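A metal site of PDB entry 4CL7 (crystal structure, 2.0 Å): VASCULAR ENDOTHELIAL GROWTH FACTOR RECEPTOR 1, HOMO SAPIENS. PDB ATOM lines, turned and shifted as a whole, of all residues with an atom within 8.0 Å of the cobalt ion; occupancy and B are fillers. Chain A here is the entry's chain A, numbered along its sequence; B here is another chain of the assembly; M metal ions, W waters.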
ATOM      1  N   ILE A  14     -31.564 -28.171 -20.147  1.00  0.00           N
ATOM      2  CA  ILE A  14     -31.913 -26.983 -20.923  1.00  0.00           C
ATOM      3  C   ILE A  14     -32.599 -27.345 -22.220  1.00  0.00           C
ATOM      4  O   ILE A  14     -32.113 -28.203 -22.965  1.00  0.00           O
ATOM      5  CB  ILE A  14     -30.664 -26.155 -21.260  1.00  0.00           C
ATOM      6  CG1 ILE A  14     -29.922 -25.761 -19.981  1.00  0.00           C
ATOM      7  CG2 ILE A  14     -31.068 -24.925 -22.070  1.00  0.00           C
ATOM      8  CD1 ILE A  14     -30.798 -25.015 -18.997  1.00  0.00           C
ATOM      9  N   ILE A  15     -33.726 -26.709 -22.502  1.00  0.00           N
ATOM     10  CA  ILE A  15     -34.428 -26.946 -23.765  1.00  0.00           C
ATOM     11  C   ILE A  15     -34.607 -25.624 -24.519  1.00  0.00           C
ATOM     12  O   ILE A  15     -35.206 -24.696 -24.000  1.00  0.00           O
ATOM     13  CB  ILE A  15     -35.823 -27.565 -23.531  1.00  0.00           C
ATOM     14  CG1 ILE A  15     -35.725 -28.842 -22.688  1.00  0.00           C
ATOM     15  CG2 ILE A  15     -36.504 -27.829 -24.872  1.00  0.00           C
ATOM     16  CD1 ILE A  15     -35.085 -30.015 -23.416  1.00  0.00           C
ATOM     17  N   HIS A  16     -34.076 -25.534 -25.734  1.00  0.00           N
ATOM     18  CA  HIS A  16     -34.257 -24.328 -26.542  1.00  0.00           C
ATOM     19  C   HIS A  16     -35.672 -24.340 -27.110  1.00  0.00           C
ATOM     20  O   HIS A  16     -36.151 -25.369 -27.596  1.00  0.00           O
ATOM     21  CB  HIS A  16     -33.195 -24.239 -27.654  1.00  0.00           C
ATOM     22  CG  HIS A  16     -31.840 -23.826 -27.149  1.00  0.00           C
ATOM     23  ND1 HIS A  16     -30.987 -24.701 -26.505  1.00  0.00           N
ATOM     24  CD2 HIS A  16     -31.220 -22.625 -27.151  1.00  0.00           C
ATOM     25  CE1 HIS A  16     -29.896 -24.058 -26.150  1.00  0.00           C
ATOM     26  NE2 HIS A  16     -30.001 -22.803 -26.534  1.00  0.00           N
ATOM     27  N   MET A  17     -36.362 -23.207 -27.000  1.00  0.00           N
ATOM     28  CA  MET A  17     -37.731 -23.107 -27.516  1.00  0.00           C
ATOM     29  C   MET A  17     -37.939 -21.874 -28.407  1.00  0.00           C
ATOM     30  O   MET A  17     -37.222 -20.884 -28.283  1.00  0.00           O
ATOM     31  CB  MET A  17     -38.741 -23.113 -26.358  1.00  0.00           C
ATOM     32  CG  MET A  17     -38.711 -21.872 -25.503  1.00  0.00           C
ATOM     33  SD  MET A  17     -39.763 -20.568 -26.167  1.00  0.00           S
ATOM     34  CE  MET A  17     -41.385 -21.195 -25.726  1.00  0.00           C
ATOM     35  N   HIS A  92     -35.925 -22.157 -22.732  1.00  0.00           N
ATOM     36  CA  HIS A  92     -34.975 -21.080 -22.896  1.00  0.00           C
ATOM     37  C   HIS A  92     -35.123 -20.521 -24.302  1.00  0.00           C
ATOM     38  O   HIS A  92     -35.134 -21.277 -25.277  1.00  0.00           O
ATOM     39  CB  HIS A  92     -33.567 -21.652 -22.649  1.00  0.00           C
ATOM     40  CG  HIS A  92     -32.456 -20.868 -23.266  1.00  0.00           C
ATOM     41  ND1 HIS A  92     -32.248 -19.533 -23.001  1.00  0.00           N
ATOM     42  CD2 HIS A  92     -31.477 -21.245 -24.115  1.00  0.00           C
ATOM     43  CE1 HIS A  92     -31.190 -19.112 -23.684  1.00  0.00           C
ATOM     44  NE2 HIS A  92     -30.707 -20.138 -24.365  1.00  0.00           N
ATOM     45  N   ARG A  93     -35.287 -19.212 -24.397  1.00  0.00           N
ATOM     46  CA  ARG A  93     -35.420 -18.531 -25.670  1.00  0.00           C
ATOM     47  C   ARG A  93     -34.044 -18.025 -26.069  1.00  0.00           C
ATOM     48  O   ARG A  93     -33.420 -17.274 -25.320  1.00  0.00           O
ATOM     49  CB  ARG A  93     -36.359 -17.339 -25.524  1.00  0.00           C
ATOM     50  CG  ARG A  93     -37.554 -17.343 -26.470  1.00  0.00           C
ATOM     51  CD  ARG A  93     -38.341 -16.029 -26.370  1.00  0.00           C
ATOM     52  NE  ARG A  93     -37.507 -14.886 -26.729  1.00  0.00           N
ATOM     53  CZ  ARG A  93     -37.943 -13.628 -26.813  1.00  0.00           C
ATOM     54  NH1 ARG A  93     -39.220 -13.341 -26.551  1.00  0.00           N
ATOM     55  NH2 ARG A  93     -37.107 -12.665 -27.156  1.00  0.00           N
ATOM     56  N   GLN A  94     -33.578 -18.440 -27.240  1.00  0.00           N
ATOM     57  CA  GLN A  94     -32.260 -18.049 -27.751  1.00  0.00           C
ATOM     58  C   GLN A  94     -31.975 -16.548 -27.625  1.00  0.00           C
ATOM     59  O   GLN A  94     -30.931 -16.136 -27.113  1.00  0.00           O
ATOM     60  CB  GLN A  94     -32.096 -18.487 -29.215  1.00  0.00           C
ATOM     61  CG  GLN A  94     -32.106 -19.992 -29.437  1.00  0.00           C
ATOM     62  CD  GLN A  94     -33.497 -20.561 -29.726  1.00  0.00           C
ATOM     63  OE1 GLN A  94     -34.507 -20.016 -29.272  1.00  0.00           O
ATOM     64  NE2 GLN A  94     -33.551 -21.647 -30.469  1.00  0.00           N
ATOM     65  OXT GLN A  94     -32.780 -15.696 -28.025  1.00  0.00           O
ATOM     66  N   ILE B  14     -30.233 -18.514 -16.852  1.00  0.00           N
ATOM     67  CA  ILE B  14     -29.417 -19.046 -17.944  1.00  0.00           C
ATOM     68  C   ILE B  14     -28.491 -17.973 -18.501  1.00  0.00           C
ATOM     69  O   ILE B  14     -28.915 -16.857 -18.797  1.00  0.00           O
ATOM     70  CB  ILE B  14     -30.287 -19.611 -19.091  1.00  0.00           C
ATOM     71  CG1 ILE B  14     -31.037 -20.857 -18.601  1.00  0.00           C
ATOM     72  CG2 ILE B  14     -29.424 -19.930 -20.307  1.00  0.00           C
ATOM     73  CD1 ILE B  14     -32.040 -21.418 -19.600  1.00  0.00           C
ATOM     74  N   ILE B  15     -27.207 -18.315 -18.634  1.00  0.00           N
ATOM     75  CA  ILE B  15     -26.253 -17.406 -19.259  1.00  0.00           C
ATOM     76  C   ILE B  15     -25.436 -18.086 -20.371  1.00  0.00           C
ATOM     77  O   ILE B  15     -25.025 -19.251 -20.259  1.00  0.00           O
ATOM     78  CB  ILE B  15     -25.331 -16.748 -18.219  1.00  0.00           C
ATOM     79  CG1 ILE B  15     -24.548 -17.797 -17.446  1.00  0.00           C
ATOM     80  CG2 ILE B  15     -26.133 -15.905 -17.223  1.00  0.00           C
ATOM     81  CD1 ILE B  15     -23.841 -17.222 -16.231  1.00  0.00           C
ATOM     82  N   HIS B  16     -25.220 -17.369 -21.455  1.00  0.00           N
ATOM     83  CA  HIS B  16     -24.498 -17.920 -22.590  1.00  0.00           C
ATOM     84  C   HIS B  16     -23.023 -17.653 -22.404  1.00  0.00           C
ATOM     85  O   HIS B  16     -22.631 -16.592 -21.918  1.00  0.00           O
ATOM     86  CB  HIS B  16     -24.973 -17.273 -23.889  1.00  0.00           C
ATOM     87  CG  HIS B  16     -26.221 -17.874 -24.444  1.00  0.00           C
ATOM     88  ND1 HIS B  16     -27.231 -17.108 -24.993  1.00  0.00           N
ATOM     89  CD2 HIS B  16     -26.634 -19.166 -24.542  1.00  0.00           C
ATOM     90  CE1 HIS B  16     -28.208 -17.908 -25.403  1.00  0.00           C
ATOM     91  NE2 HIS B  16     -27.876 -19.150 -25.134  1.00  0.00           N
ATOM     92  N   MET B  17     -22.203 -18.618 -22.798  1.00  0.00           N
ATOM     93  CA  MET B  17     -20.758 -18.411 -22.855  1.00  0.00           C
ATOM     94  C   MET B  17     -20.237 -18.790 -24.236  1.00  0.00           C
ATOM     95  O   MET B  17     -20.930 -19.465 -25.013  1.00  0.00           O
ATOM     96  CB  MET B  17     -20.063 -19.268 -21.801  1.00  0.00           C
ATOM     97  CG  MET B  17     -20.483 -20.717 -21.856  1.00  0.00           C
ATOM     98  SD  MET B  17     -19.335 -21.824 -21.024  1.00  0.00           S
ATOM     99  CE  MET B  17     -18.063 -21.937 -22.301  1.00  0.00           C
ATOM    100  N   THR B  91     -24.826 -22.305 -17.359  1.00  0.00           N
ATOM    101  CA  THR B  91     -24.124 -21.800 -18.531  1.00  0.00           C
ATOM    102  C   THR B  91     -24.206 -22.804 -19.669  1.00  0.00           C
ATOM    103  O   THR B  91     -24.133 -24.008 -19.452  1.00  0.00           O
ATOM    104  CB  THR B  91     -22.645 -21.575 -18.229  1.00  0.00           C
ATOM    105  OG1 THR B  91     -22.115 -22.790 -17.691  1.00  0.00           O
ATOM    106  CG2 THR B  91     -22.478 -20.463 -17.192  1.00  0.00           C
ATOM    107  N   HIS B  92     -24.340 -22.306 -20.895  1.00  0.00           N
ATOM    108  CA  HIS B  92     -24.131 -23.156 -22.061  1.00  0.00           C
ATOM    109  C   HIS B  92     -23.698 -22.293 -23.228  1.00  0.00           C
ATOM    110  O   HIS B  92     -23.761 -21.057 -23.157  1.00  0.00           O
ATOM    111  CB  HIS B  92     -25.372 -23.974 -22.393  1.00  0.00           C
ATOM    112  CG  HIS B  92     -26.495 -23.163 -22.963  1.00  0.00           C
ATOM    113  ND1 HIS B  92     -27.397 -22.486 -22.180  1.00  0.00           N
ATOM    114  CD2 HIS B  92     -26.839 -22.901 -24.245  1.00  0.00           C
ATOM    115  CE1 HIS B  92     -28.259 -21.855 -22.950  1.00  0.00           C
ATOM    116  NE2 HIS B  92     -27.938 -22.094 -24.209  1.00  0.00           N
ATOM    117  N   ARG B  93     -23.213 -22.929 -24.287  1.00  0.00           N
ATOM    118  CA  ARG B  93     -22.579 -22.192 -25.357  1.00  0.00           C
ATOM    119  C   ARG B  93     -23.575 -21.402 -26.193  1.00  0.00           C
ATOM    120  O   ARG B  93     -24.674 -21.866 -26.452  1.00  0.00           O
ATOM    121  CB  ARG B  93     -21.722 -23.110 -26.234  1.00  0.00           C
ATOM    122  CG  ARG B  93     -20.419 -23.524 -25.549  1.00  0.00           C
ATOM    123  CD  ARG B  93     -19.754 -24.658 -26.305  1.00  0.00           C
ATOM    124  NE  ARG B  93     -20.610 -25.839 -26.314  1.00  0.00           N
ATOM    125  CZ  ARG B  93     -20.162 -27.083 -26.314  1.00  0.00           C
ATOM    126  NH1 ARG B  93     -18.856 -27.328 -26.300  1.00  0.00           N
ATOM    127  NH2 ARG B  93     -21.018 -28.097 -26.326  1.00  0.00           N
ATOM    128  N   GLN B  94     -23.154 -20.198 -26.568  1.00  0.00           N
ATOM    129  CA  GLN B  94     -23.933 -19.292 -27.382  1.00  0.00           C
ATOM    130  C   GLN B  94     -24.126 -19.892 -28.753  1.00  0.00           C
ATOM    131  O   GLN B  94     -25.205 -19.789 -29.346  1.00  0.00           O
ATOM    132  CB  GLN B  94     -23.177 -17.960 -27.501  1.00  0.00           C
ATOM    133  CG  GLN B  94     -23.817 -16.955 -28.407  1.00  0.00           C
ATOM    134  CD  GLN B  94     -24.951 -16.221 -27.751  1.00  0.00           C
ATOM    135  OE1 GLN B  94     -24.744 -15.215 -27.095  1.00  0.00           O
ATOM    136  NE2 GLN B  94     -26.161 -16.741 -27.915  1.00  0.00           N
ATOM    137  OXT GLN B  94     -23.190 -20.502 -29.305  1.00  0.00           O
HETATM  138 CO    CO M   1     -28.983 -20.939 -25.751  1.00  0.00          CO
HETATM  139  O   HOH W   1     -27.336 -21.458 -27.194  1.00  0.00           O
HETATM  140  O   HOH W   2     -29.915 -19.630 -27.302  1.00  0.00           O
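The cobalt ion is bound by NE2 of His 92 of chain B (2.2 Å), NE2 of His 16 of chain B (2.2 Å), water W2 (2.2 Å), water W1 (2.3 Å), NE2 of His 16 of chain A (2.3 Å) and NE2 of His 92 of chain A (2.4 Å).
The cobalt ion has six donor atoms within binding distance.
Within 4 Å of the cobalt ion: His 16 of chain A, His 92 of chain A, His 16 of chain B and His 92 of chain B.
The nearest printed residue that does not touch the cobalt ion is Arg 93 of chain B (4.5 Å).
O of Ile 15 of chain B lies within hydrogen-bond range of N of His 92 of chain B (3.2 Å).
NE2 of Gln 94 of chain B lies within hydrogen-bond range of ND1 of His 16 of chain B, at 3.1 Å.
The backbone NH of His 92 of chain A is in hydrogen-bond range of the backbone carbonyl oxygen of Ile 15 of chain A (2.9 Å).
The backbone NH (N) of Met 17 of chain A sits at hydrogen-bond distance from the backbone carbonyl oxygen (O) of His 92 of chain A (2.9 Å).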
